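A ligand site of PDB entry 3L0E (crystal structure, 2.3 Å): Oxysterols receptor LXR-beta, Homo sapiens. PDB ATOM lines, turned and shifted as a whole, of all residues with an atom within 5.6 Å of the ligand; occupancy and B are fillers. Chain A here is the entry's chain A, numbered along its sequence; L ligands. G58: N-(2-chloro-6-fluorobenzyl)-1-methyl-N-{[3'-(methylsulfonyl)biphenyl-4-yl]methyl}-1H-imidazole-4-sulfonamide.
NH1 of Arg 111 is in hydrogen-bond range of O3 of the ligand. N of Leu 122 is in hydrogen-bond range of O3 of the ligand, 3.0 Å away.
Residues that only touch the ligand: Phe 60 (3.2 Å), Phe 63 (3.5 Å), Thr 64 (3.6 Å), Leu 66 (3.4 Å), Ala 67 (3.3 Å), Ile 69 (3.9 Å), Ser 70 (3.5 Å), Ile 101 (3.1 Å), Met 104 (3.7 Å), Glu 107 (3.7 Å), Thr 108 (3.3 Å), Phe 121 (3.2 Å), Phe 132 (3.4 Å), Ala 135 (3.5 Å), Gly 136 (3.3 Å), Leu 137 (3.5 Å), Phe 141 (3.97 Å), His 227 (3.3 Å), Leu 234 (3.5 Å), Leu 245 (3.5 Å) and Trp 249 (3.5 Å). Hydrophobic or aromatic side chains within 4 Å of the ligand: Phe 60, Phe 63, Leu 66, Ala 67, Ile 69, Ile 101, Met 104, Phe 121, Leu 122, Phe 132, Leu 137, Phe 141, His 227, Leu 234, Leu 245 and Trp 249. Of the 31 residues printed, 23 come within 4 Å of the ligand.
The side-chain carboxylate (OE1) of Glu 107 lies within salt-bridge range of the guanidinium group (NH2) of Arg 111. The backbone NH (N) of Thr 120 is in hydrogen-bond range of the backbone carbonyl oxygen (O) of Arg 111, at 3.2 Å. The side-chain hydroxyl (OG1) of Thr 108 is in hydrogen-bond range of the backbone carbonyl oxygen (O) of Met 104 (2.7 Å). N of Leu 137 lies within hydrogen-bond range of O of Phe 132, at 3.3 Å.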
ATOM      1  N   SER A  34     -24.520   8.086 -21.635  1.00  0.00           N
ATOM      2  CA  SER A  34     -23.574   9.214 -21.665  1.00  0.00           C
ATOM      3  C   SER A  34     -23.199   9.670 -23.092  1.00  0.00           C
ATOM      4  O   SER A  34     -23.166  10.880 -23.373  1.00  0.00           O
ATOM      5  CB  SER A  34     -22.276   8.852 -20.927  1.00  0.00           C
ATOM      6  OG  SER A  34     -22.537   8.386 -19.620  1.00  0.00           O
ATOM      7  N   PHE A  60     -12.698  24.935 -17.943  1.00  0.00           N
ATOM      8  CA  PHE A  60     -13.228  24.563 -16.614  1.00  0.00           C
ATOM      9  C   PHE A  60     -14.641  23.948 -16.688  1.00  0.00           C
ATOM     10  O   PHE A  60     -14.904  22.897 -16.104  1.00  0.00           O
ATOM     11  CB  PHE A  60     -13.209  25.784 -15.693  1.00  0.00           C
ATOM     12  CG  PHE A  60     -13.705  25.513 -14.295  1.00  0.00           C
ATOM     13  CD1 PHE A  60     -12.896  24.892 -13.360  1.00  0.00           C
ATOM     14  CD2 PHE A  60     -14.986  25.900 -13.921  1.00  0.00           C
ATOM     15  CE1 PHE A  60     -13.372  24.649 -12.071  1.00  0.00           C
ATOM     16  CE2 PHE A  60     -15.445  25.657 -12.631  1.00  0.00           C
ATOM     17  CZ  PHE A  60     -14.622  25.026 -11.714  1.00  0.00           C
ATOM     18  N   PHE A  63     -14.814  20.309 -18.223  1.00  0.00           N
ATOM     19  CA  PHE A  63     -14.471  19.317 -17.197  1.00  0.00           C
ATOM     20  C   PHE A  63     -15.552  19.072 -16.160  1.00  0.00           C
ATOM     21  O   PHE A  63     -15.833  17.916 -15.835  1.00  0.00           O
ATOM     22  CB  PHE A  63     -13.168  19.711 -16.482  1.00  0.00           C
ATOM     23  CG  PHE A  63     -11.951  19.026 -17.017  1.00  0.00           C
ATOM     24  CD1 PHE A  63     -11.581  19.189 -18.351  1.00  0.00           C
ATOM     25  CD2 PHE A  63     -11.188  18.213 -16.200  1.00  0.00           C
ATOM     26  CE1 PHE A  63     -10.466  18.558 -18.851  1.00  0.00           C
ATOM     27  CE2 PHE A  63     -10.066  17.584 -16.708  1.00  0.00           C
ATOM     28  CZ  PHE A  63      -9.713  17.762 -18.039  1.00  0.00           C
ATOM     29  N   THR A  64     -16.153  20.140 -15.625  1.00  0.00           N
ATOM     30  CA  THR A  64     -17.182  19.955 -14.595  1.00  0.00           C
ATOM     31  C   THR A  64     -18.458  19.330 -15.186  1.00  0.00           C
ATOM     32  O   THR A  64     -19.228  18.663 -14.479  1.00  0.00           O
ATOM     33  CB  THR A  64     -17.521  21.259 -13.826  1.00  0.00           C
ATOM     34  OG1 THR A  64     -18.178  22.186 -14.683  1.00  0.00           O
ATOM     35  CG2 THR A  64     -16.262  21.908 -13.243  1.00  0.00           C
ATOM     36  N   LEU A  66     -18.265  17.022 -17.735  1.00  0.00           N
ATOM     37  CA  LEU A  66     -17.881  15.613 -17.847  1.00  0.00           C
ATOM     38  C   LEU A  66     -18.023  14.946 -16.478  1.00  0.00           C
ATOM     39  O   LEU A  66     -18.453  13.781 -16.378  1.00  0.00           O
ATOM     40  CB  LEU A  66     -16.449  15.468 -18.390  1.00  0.00           C
ATOM     41  CG  LEU A  66     -16.110  15.964 -19.810  1.00  0.00           C
ATOM     42  CD1 LEU A  66     -14.620  15.843 -20.081  1.00  0.00           C
ATOM     43  CD2 LEU A  66     -16.927  15.229 -20.884  1.00  0.00           C
ATOM     44  N   ALA A  67     -17.656  15.671 -15.417  1.00  0.00           N
ATOM     45  CA  ALA A  67     -17.794  15.163 -14.043  1.00  0.00           C
ATOM     46  C   ALA A  67     -19.265  14.847 -13.737  1.00  0.00           C
ATOM     47  O   ALA A  67     -19.549  13.797 -13.185  1.00  0.00           O
ATOM     48  CB  ALA A  67     -17.208  16.141 -13.009  1.00  0.00           C
ATOM     49  N   ILE A  69     -21.740  14.097 -15.906  1.00  0.00           N
ATOM     50  CA  ILE A  69     -22.064  12.870 -16.659  1.00  0.00           C
ATOM     51  C   ILE A  69     -21.529  11.606 -15.957  1.00  0.00           C
ATOM     52  O   ILE A  69     -22.231  10.583 -15.878  1.00  0.00           O
ATOM     53  CB  ILE A  69     -21.498  12.910 -18.087  1.00  0.00           C
ATOM     54  CG1 ILE A  69     -22.167  14.023 -18.903  1.00  0.00           C
ATOM     55  CG2 ILE A  69     -21.717  11.581 -18.763  1.00  0.00           C
ATOM     56  CD1 ILE A  69     -21.404  14.380 -20.171  1.00  0.00           C
ATOM     57  N   SER A  70     -20.290  11.679 -15.464  1.00  0.00           N
ATOM     58  CA  SER A  70     -19.689  10.594 -14.683  1.00  0.00           C
ATOM     59  C   SER A  70     -20.530  10.235 -13.444  1.00  0.00           C
ATOM     60  O   SER A  70     -20.769   9.065 -13.207  1.00  0.00           O
ATOM     61  CB  SER A  70     -18.254  10.943 -14.285  1.00  0.00           C
ATOM     62  OG  SER A  70     -17.610   9.842 -13.673  1.00  0.00           O
ATOM     63  N   GLU A  73     -23.632   8.342 -14.693  1.00  0.00           N
ATOM     64  CA  GLU A  73     -23.241   6.948 -14.956  1.00  0.00           C
ATOM     65  C   GLU A  73     -23.117   6.103 -13.689  1.00  0.00           C
ATOM     66  O   GLU A  73     -23.524   4.941 -13.662  1.00  0.00           O
ATOM     67  CB  GLU A  73     -21.890   6.895 -15.652  1.00  0.00           C
ATOM     68  CG  GLU A  73     -21.881   7.248 -17.125  1.00  0.00           C
ATOM     69  CD  GLU A  73     -20.520   6.964 -17.766  1.00  0.00           C
ATOM     70  OE1 GLU A  73     -19.557   6.683 -16.985  1.00  0.00           O
ATOM     71  OE2 GLU A  73     -20.410   7.016 -19.030  1.00  0.00           O
ATOM     72  N   ILE A 101     -16.102   9.957  -5.940  1.00  0.00           N
ATOM     73  CA  ILE A 101     -14.747  10.325  -6.330  1.00  0.00           C
ATOM     74  C   ILE A 101     -13.882   9.095  -6.668  1.00  0.00           C
ATOM     75  O   ILE A 101     -13.095   9.116  -7.627  1.00  0.00           O
ATOM     76  CB  ILE A 101     -14.071  11.207  -5.245  1.00  0.00           C
ATOM     77  CG1 ILE A 101     -12.734  11.741  -5.783  1.00  0.00           C
ATOM     78  CG2 ILE A 101     -13.862  10.449  -3.907  1.00  0.00           C
ATOM     79  CD1 ILE A 101     -12.895  12.533  -7.015  1.00  0.00           C
ATOM     80  N   MET A 104     -15.039   7.539  -9.949  1.00  0.00           N
ATOM     81  CA  MET A 104     -14.585   8.472 -10.992  1.00  0.00           C
ATOM     82  C   MET A 104     -13.110   8.232 -11.348  1.00  0.00           C
ATOM     83  O   MET A 104     -12.735   8.291 -12.517  1.00  0.00           O
ATOM     84  CB  MET A 104     -14.726   9.923 -10.539  1.00  0.00           C
ATOM     85  CG  MET A 104     -16.106  10.541 -10.686  1.00  0.00           C
ATOM     86  SD  MET A 104     -16.108  12.236 -10.048  1.00  0.00           S
ATOM     87  CE  MET A 104     -17.751  12.794 -10.438  1.00  0.00           C
ATOM     88  N   LEU A 105     -12.284   8.005 -10.321  1.00  0.00           N
ATOM     89  CA  LEU A 105     -10.835   7.758 -10.499  1.00  0.00           C
ATOM     90  C   LEU A 105     -10.516   6.365 -11.080  1.00  0.00           C
ATOM     91  O   LEU A 105      -9.602   6.228 -11.878  1.00  0.00           O
ATOM     92  CB  LEU A 105     -10.092   7.979  -9.168  1.00  0.00           C
ATOM     93  CG  LEU A 105      -9.973   9.431  -8.626  1.00  0.00           C
ATOM     94  CD1 LEU A 105      -9.730   9.459  -7.103  1.00  0.00           C
ATOM     95  CD2 LEU A 105      -8.885  10.220  -9.349  1.00  0.00           C
ATOM     96  N   GLU A 107     -12.564   4.872 -13.133  1.00  0.00           N
ATOM     97  CA  GLU A 107     -13.031   5.070 -14.505  1.00  0.00           C
ATOM     98  C   GLU A 107     -12.078   5.912 -15.344  1.00  0.00           C
ATOM     99  O   GLU A 107     -11.947   5.694 -16.541  1.00  0.00           O
ATOM    100  CB  GLU A 107     -14.412   5.740 -14.505  1.00  0.00           C
ATOM    101  CG  GLU A 107     -15.573   4.783 -14.426  1.00  0.00           C
ATOM    102  CD  GLU A 107     -15.593   3.791 -15.570  1.00  0.00           C
ATOM    103  OE1 GLU A 107     -15.153   4.133 -16.728  1.00  0.00           O
ATOM    104  OE2 GLU A 107     -16.037   2.660 -15.310  1.00  0.00           O
ATOM    105  N   THR A 108     -11.436   6.892 -14.705  1.00  0.00           N
ATOM    106  CA  THR A 108     -10.350   7.641 -15.321  1.00  0.00           C
ATOM    107  C   THR A 108      -9.161   6.710 -15.623  1.00  0.00           C
ATOM    108  O   THR A 108      -8.584   6.764 -16.714  1.00  0.00           O
ATOM    109  CB  THR A 108      -9.883   8.797 -14.409  1.00  0.00           C
ATOM    110  OG1 THR A 108     -11.003   9.621 -14.077  1.00  0.00           O
ATOM    111  CG2 THR A 108      -8.809   9.642 -15.091  1.00  0.00           C
ATOM    112  N   ARG A 111      -9.592   4.628 -18.648  1.00  0.00           N
ATOM    113  CA  ARG A 111      -9.479   5.409 -19.891  1.00  0.00           C
ATOM    114  C   ARG A 111      -8.091   6.003 -20.153  1.00  0.00           C
ATOM    115  O   ARG A 111      -7.895   6.746 -21.133  1.00  0.00           O
ATOM    116  CB  ARG A 111     -10.496   6.544 -19.871  1.00  0.00           C
ATOM    117  CG  ARG A 111     -11.914   6.070 -19.898  1.00  0.00           C
ATOM    118  CD  ARG A 111     -12.834   7.055 -19.271  1.00  0.00           C
ATOM    119  NE  ARG A 111     -14.112   6.413 -19.007  1.00  0.00           N
ATOM    120  CZ  ARG A 111     -15.124   6.376 -19.861  1.00  0.00           C
ATOM    121  NH1 ARG A 111     -15.065   6.955 -21.056  1.00  0.00           N
ATOM    122  NH2 ARG A 111     -16.237   5.737 -19.495  1.00  0.00           N
ATOM    123  N   THR A 120      -8.865   9.592 -22.178  1.00  0.00           N
ATOM    124  CA  THR A 120      -9.929   9.900 -23.146  1.00  0.00           C
ATOM    125  C   THR A 120     -11.287   9.794 -22.485  1.00  0.00           C
ATOM    126  O   THR A 120     -11.713   8.711 -22.091  1.00  0.00           O
ATOM    127  CB  THR A 120      -9.872   8.964 -24.396  1.00  0.00           C
ATOM    128  OG1 THR A 120      -8.556   9.010 -24.961  1.00  0.00           O
ATOM    129  CG2 THR A 120     -10.881   9.411 -25.482  1.00  0.00           C
ATOM    130  N   PHE A 121     -11.972  10.931 -22.341  1.00  0.00           N
ATOM    131  CA  PHE A 121     -13.324  10.954 -21.762  1.00  0.00           C
ATOM    132  C   PHE A 121     -14.365  10.849 -22.887  1.00  0.00           C
ATOM    133  O   PHE A 121     -14.153  11.413 -23.968  1.00  0.00           O
ATOM    134  CB  PHE A 121     -13.511  12.230 -20.950  1.00  0.00           C
ATOM    135  CG  PHE A 121     -12.623  12.336 -19.728  1.00  0.00           C
ATOM    136  CD1 PHE A 121     -12.617  11.334 -18.765  1.00  0.00           C
ATOM    137  CD2 PHE A 121     -11.800  13.442 -19.532  1.00  0.00           C
ATOM    138  CE1 PHE A 121     -11.803  11.431 -17.635  1.00  0.00           C
ATOM    139  CE2 PHE A 121     -11.003  13.548 -18.414  1.00  0.00           C
ATOM    140  CZ  PHE A 121     -11.002  12.541 -17.457  1.00  0.00           C
ATOM    141  N   LEU A 122     -15.466  10.123 -22.642  1.00  0.00           N
ATOM    142  CA  LEU A 122     -16.495   9.852 -23.680  1.00  0.00           C
ATOM    143  C   LEU A 122     -15.849   9.260 -24.951  1.00  0.00           C
ATOM    144  O   LEU A 122     -14.888   8.493 -24.840  1.00  0.00           O
ATOM    145  CB  LEU A 122     -17.355  11.112 -23.950  1.00  0.00           C
ATOM    146  CG  LEU A 122     -18.203  11.635 -22.751  1.00  0.00           C
ATOM    147  CD1 LEU A 122     -19.087  12.808 -23.145  1.00  0.00           C
ATOM    148  CD2 LEU A 122     -19.064  10.532 -22.144  1.00  0.00           C
ATOM    149  N   PHE A 132      -5.292  19.008 -18.142  1.00  0.00           N
ATOM    150  CA  PHE A 132      -5.897  18.964 -16.791  1.00  0.00           C
ATOM    151  C   PHE A 132      -5.580  20.249 -16.041  1.00  0.00           C
ATOM    152  O   PHE A 132      -6.416  20.772 -15.329  1.00  0.00           O
ATOM    153  CB  PHE A 132      -5.406  17.768 -15.987  1.00  0.00           C
ATOM    154  CG  PHE A 132      -6.198  16.513 -16.195  1.00  0.00           C
ATOM    155  CD1 PHE A 132      -6.353  15.973 -17.455  1.00  0.00           C
ATOM    156  CD2 PHE A 132      -6.791  15.864 -15.115  1.00  0.00           C
ATOM    157  CE1 PHE A 132      -7.077  14.834 -17.654  1.00  0.00           C
ATOM    158  CE2 PHE A 132      -7.510  14.708 -15.301  1.00  0.00           C
ATOM    159  CZ  PHE A 132      -7.663  14.188 -16.582  1.00  0.00           C
ATOM    160  N   ALA A 135      -7.675  23.073 -17.414  1.00  0.00           N
ATOM    161  CA  ALA A 135      -9.053  22.942 -16.925  1.00  0.00           C
ATOM    162  C   ALA A 135      -9.215  23.448 -15.476  1.00  0.00           C
ATOM    163  O   ALA A 135     -10.302  23.356 -14.929  1.00  0.00           O
ATOM    164  CB  ALA A 135      -9.514  21.485 -17.037  1.00  0.00           C
ATOM    165  N   GLY A 136      -8.148  23.958 -14.854  1.00  0.00           N
ATOM    166  CA  GLY A 136      -8.245  24.540 -13.503  1.00  0.00           C
ATOM    167  C   GLY A 136      -7.792  23.647 -12.355  1.00  0.00           C
ATOM    168  O   GLY A 136      -8.004  23.978 -11.184  1.00  0.00           O
ATOM    169  N   LEU A 137      -7.174  22.504 -12.666  1.00  0.00           N
ATOM    170  CA  LEU A 137      -6.715  21.554 -11.650  1.00  0.00           C
ATOM    171  C   LEU A 137      -5.268  21.847 -11.255  1.00  0.00           C
ATOM    172  O   LEU A 137      -4.470  22.319 -12.058  1.00  0.00           O
ATOM    173  CB  LEU A 137      -6.880  20.096 -12.113  1.00  0.00           C
ATOM    174  CG  LEU A 137      -8.328  19.632 -12.338  1.00  0.00           C
ATOM    175  CD1 LEU A 137      -8.425  18.403 -13.233  1.00  0.00           C
ATOM    176  CD2 LEU A 137      -9.043  19.390 -11.026  1.00  0.00           C
ATOM    177  N   PHE A 141      -2.986  17.474  -7.402  1.00  0.00           N
ATOM    178  CA  PHE A 141      -4.015  16.494  -7.727  1.00  0.00           C
ATOM    179  C   PHE A 141      -3.723  15.770  -9.041  1.00  0.00           C
ATOM    180  O   PHE A 141      -3.983  14.570  -9.167  1.00  0.00           O
ATOM    181  CB  PHE A 141      -5.372  17.181  -7.796  1.00  0.00           C
ATOM    182  CG  PHE A 141      -6.533  16.230  -7.986  1.00  0.00           C
ATOM    183  CD1 PHE A 141      -6.669  15.095  -7.181  1.00  0.00           C
ATOM    184  CD2 PHE A 141      -7.492  16.484  -8.958  1.00  0.00           C
ATOM    185  CE1 PHE A 141      -7.734  14.231  -7.358  1.00  0.00           C
ATOM    186  CE2 PHE A 141      -8.575  15.624  -9.124  1.00  0.00           C
ATOM    187  CZ  PHE A 141      -8.688  14.491  -8.324  1.00  0.00           C
ATOM    188  N   ILE A 145      -3.351  11.470  -9.867  1.00  0.00           N
ATOM    189  CA  ILE A 145      -4.319  10.912 -10.822  1.00  0.00           C
ATOM    190  C   ILE A 145      -3.610  10.106 -11.920  1.00  0.00           C
ATOM    191  O   ILE A 145      -3.953   8.955 -12.172  1.00  0.00           O
ATOM    192  CB  ILE A 145      -5.195  12.010 -11.512  1.00  0.00           C
ATOM    193  CG1 ILE A 145      -6.216  12.610 -10.535  1.00  0.00           C
ATOM    194  CG2 ILE A 145      -5.951  11.439 -12.718  1.00  0.00           C
ATOM    195  CD1 ILE A 145      -6.910  13.895 -11.072  1.00  0.00           C
ATOM    196  N   HIS A 227      -8.306  14.897  -3.379  1.00  0.00           N
ATOM    197  CA  HIS A 227      -9.403  15.602  -4.068  1.00  0.00           C
ATOM    198  C   HIS A 227     -10.172  16.610  -3.183  1.00  0.00           C
ATOM    199  O   HIS A 227     -10.522  17.694  -3.652  1.00  0.00           O
ATOM    200  CB  HIS A 227     -10.390  14.589  -4.676  1.00  0.00           C
ATOM    201  CG  HIS A 227     -11.616  15.210  -5.269  1.00  0.00           C
ATOM    202  ND1 HIS A 227     -12.805  15.314  -4.582  1.00  0.00           N
ATOM    203  CD2 HIS A 227     -11.822  15.770  -6.482  1.00  0.00           C
ATOM    204  CE1 HIS A 227     -13.697  15.893  -5.357  1.00  0.00           C
ATOM    205  NE2 HIS A 227     -13.133  16.182  -6.518  1.00  0.00           N
ATOM    206  N   GLN A 230      -8.109  19.580  -3.106  1.00  0.00           N
ATOM    207  CA  GLN A 230      -8.351  20.281  -4.392  1.00  0.00           C
ATOM    208  C   GLN A 230      -9.655  21.111  -4.352  1.00  0.00           C
ATOM    209  O   GLN A 230      -9.655  22.269  -4.783  1.00  0.00           O
ATOM    210  CB  GLN A 230      -8.357  19.275  -5.568  1.00  0.00           C
ATOM    211  CG  GLN A 230      -9.046  19.730  -6.887  1.00  0.00           C
ATOM    212  CD  GLN A 230      -8.175  20.655  -7.722  1.00  0.00           C
ATOM    213  OE1 GLN A 230      -7.219  20.220  -8.361  1.00  0.00           O
ATOM    214  NE2 GLN A 230      -8.508  21.946  -7.718  1.00  0.00           N
ATOM    215  N   VAL A 231     -10.731  20.511  -3.809  1.00  0.00           N
ATOM    216  CA  VAL A 231     -12.047  21.159  -3.678  1.00  0.00           C
ATOM    217  C   VAL A 231     -11.993  22.403  -2.762  1.00  0.00           C
ATOM    218  O   VAL A 231     -12.434  23.468  -3.167  1.00  0.00           O
ATOM    219  CB  VAL A 231     -13.156  20.160  -3.176  1.00  0.00           C
ATOM    220  CG1 VAL A 231     -14.391  20.897  -2.710  1.00  0.00           C
ATOM    221  CG2 VAL A 231     -13.528  19.174  -4.271  1.00  0.00           C
ATOM    222  N   LEU A 234     -10.199  25.149  -4.699  1.00  0.00           N
ATOM    223  CA  LEU A 234     -11.070  25.855  -5.664  1.00  0.00           C
ATOM    224  C   LEU A 234     -11.796  26.996  -4.963  1.00  0.00           C
ATOM    225  O   LEU A 234     -11.725  28.147  -5.415  1.00  0.00           O
ATOM    226  CB  LEU A 234     -12.108  24.912  -6.297  1.00  0.00           C
ATOM    227  CG  LEU A 234     -11.649  24.000  -7.437  1.00  0.00           C
ATOM    228  CD1 LEU A 234     -12.654  22.875  -7.673  1.00  0.00           C
ATOM    229  CD2 LEU A 234     -11.454  24.833  -8.703  1.00  0.00           C
ATOM    230  N   LEU A 241     -18.227  25.419  -8.844  1.00  0.00           N
ATOM    231  CA  LEU A 241     -18.631  24.030  -9.170  1.00  0.00           C
ATOM    232  C   LEU A 241     -20.160  23.964  -9.306  1.00  0.00           C
ATOM    233  O   LEU A 241     -20.876  24.589  -8.517  1.00  0.00           O
ATOM    234  CB  LEU A 241     -18.145  23.022  -8.120  1.00  0.00           C
ATOM    235  CG  LEU A 241     -16.733  22.415  -8.224  1.00  0.00           C
ATOM    236  CD1 LEU A 241     -16.585  21.276  -7.215  1.00  0.00           C
ATOM    237  CD2 LEU A 241     -16.391  21.893  -9.616  1.00  0.00           C
ATOM    238  N   LEU A 245     -22.436  18.602  -8.050  1.00  0.00           N
ATOM    239  CA  LEU A 245     -21.059  18.370  -7.573  1.00  0.00           C
ATOM    240  C   LEU A 245     -20.782  19.039  -6.201  1.00  0.00           C
ATOM    241  O   LEU A 245     -20.230  18.398  -5.304  1.00  0.00           O
ATOM    242  CB  LEU A 245     -20.015  18.843  -8.621  1.00  0.00           C
ATOM    243  CG  LEU A 245     -19.889  18.106  -9.961  1.00  0.00           C
ATOM    244  CD1 LEU A 245     -18.571  18.537 -10.677  1.00  0.00           C
ATOM    245  CD2 LEU A 245     -19.937  16.592  -9.813  1.00  0.00           C
ATOM    246  N   TRP A 249     -20.218  16.585  -2.776  1.00  0.00           N
ATOM    247  CA  TRP A 249     -18.939  16.758  -2.087  1.00  0.00           C
ATOM    248  C   TRP A 249     -18.983  17.746  -0.933  1.00  0.00           C
ATOM    249  O   TRP A 249     -17.927  18.158  -0.452  1.00  0.00           O
ATOM    250  CB  TRP A 249     -17.830  17.146  -3.075  1.00  0.00           C
ATOM    251  CG  TRP A 249     -17.548  16.073  -4.087  1.00  0.00           C
ATOM    252  CD1 TRP A 249     -17.641  14.722  -3.895  1.00  0.00           C
ATOM    253  CD2 TRP A 249     -17.124  16.257  -5.436  1.00  0.00           C
ATOM    254  NE1 TRP A 249     -17.300  14.055  -5.044  1.00  0.00           N
ATOM    255  CE2 TRP A 249     -16.969  14.980  -6.007  1.00  0.00           C
ATOM    256  CE3 TRP A 249     -16.839  17.392  -6.221  1.00  0.00           C
ATOM    257  CZ2 TRP A 249     -16.566  14.795  -7.338  1.00  0.00           C
ATOM    258  CZ3 TRP A 249     -16.433  17.207  -7.522  1.00  0.00           C
ATOM    259  CH2 TRP A 249     -16.297  15.911  -8.074  1.00  0.00           C
HETATM  260  C1  G58 L   1     -10.966  22.596 -11.328  1.00  0.00           C
HETATM  261  F1  G58 L   1     -10.455  15.455 -13.855  1.00  0.00           F
HETATM  262  N1  G58 L   1     -11.845  21.506 -11.689  1.00  0.00           N
HETATM  263  O1  G58 L   1     -13.843  18.278  -9.679  1.00  0.00           O
HETATM  264  S1  G58 L   1     -13.977  18.329 -11.126  1.00  0.00           S
HETATM  265 CL1  G58 L   1     -12.623  14.483  -9.412  1.00  0.00          CL
HETATM  266  C2  G58 L   1     -12.317  21.230 -12.936  1.00  0.00           C
HETATM  267  N2  G58 L   1     -13.087  20.166 -12.940  1.00  0.00           N
HETATM  268  O2  G58 L   1     -15.262  18.631 -11.735  1.00  0.00           O
HETATM  269  S2  G58 L   1     -16.555  10.499 -18.890  1.00  0.00           S
HETATM  270  C3  G58 L   1     -13.093  19.744 -11.631  1.00  0.00           C
HETATM  271  N3  G58 L   1     -13.245  16.912 -11.857  1.00  0.00           N
HETATM  272  O3  G58 L   1     -15.936   9.471 -19.708  1.00  0.00           O
HETATM  273  C4  G58 L   1     -12.335  20.557 -10.829  1.00  0.00           C
HETATM  274  O4  G58 L   1     -17.954  10.434 -18.496  1.00  0.00           O
HETATM  275  C5  G58 L   1     -13.540  16.821 -13.306  1.00  0.00           C
HETATM  276  C6  G58 L   1     -13.876  15.465 -13.822  1.00  0.00           C
HETATM  277  C7  G58 L   1     -14.383  14.452 -13.033  1.00  0.00           C
HETATM  278  C8  G58 L   1     -14.660  13.220 -13.573  1.00  0.00           C
HETATM  279  C9  G58 L   1     -14.447  12.972 -14.910  1.00  0.00           C
HETATM  280  C10 G58 L   1     -13.941  13.998 -15.695  1.00  0.00           C
HETATM  281  C11 G58 L   1     -13.658  15.223 -15.152  1.00  0.00           C
HETATM  282  C12 G58 L   1     -14.740  11.700 -15.528  1.00  0.00           C
HETATM  283  C13 G58 L   1     -14.375  10.498 -14.955  1.00  0.00           C
HETATM  284  C14 G58 L   1     -14.676   9.302 -15.560  1.00  0.00           C
HETATM  285  C15 G58 L   1     -15.352   9.279 -16.766  1.00  0.00           C
HETATM  286  C16 G58 L   1     -15.688  10.489 -17.339  1.00  0.00           C
HETATM  287  C17 G58 L   1     -15.399  11.691 -16.729  1.00  0.00           C
HETATM  288  C18 G58 L   1     -16.422  12.110 -19.584  1.00  0.00           C
HETATM  289  C19 G58 L   1     -11.797  16.500 -11.528  1.00  0.00           C
HETATM  290  C20 G58 L   1     -11.470  15.027 -11.774  1.00  0.00           C
HETATM  291  C21 G58 L   1     -10.831  14.579 -12.917  1.00  0.00           C
HETATM  292  C22 G58 L   1     -10.560  13.243 -13.135  1.00  0.00           C
HETATM  293  C23 G58 L   1     -10.923  12.296 -12.205  1.00  0.00           C
HETATM  294  C24 G58 L   1     -11.550  12.701 -11.062  1.00  0.00           C
HETATM  295  C25 G58 L   1     -11.813  14.035 -10.866  1.00  0.00           C
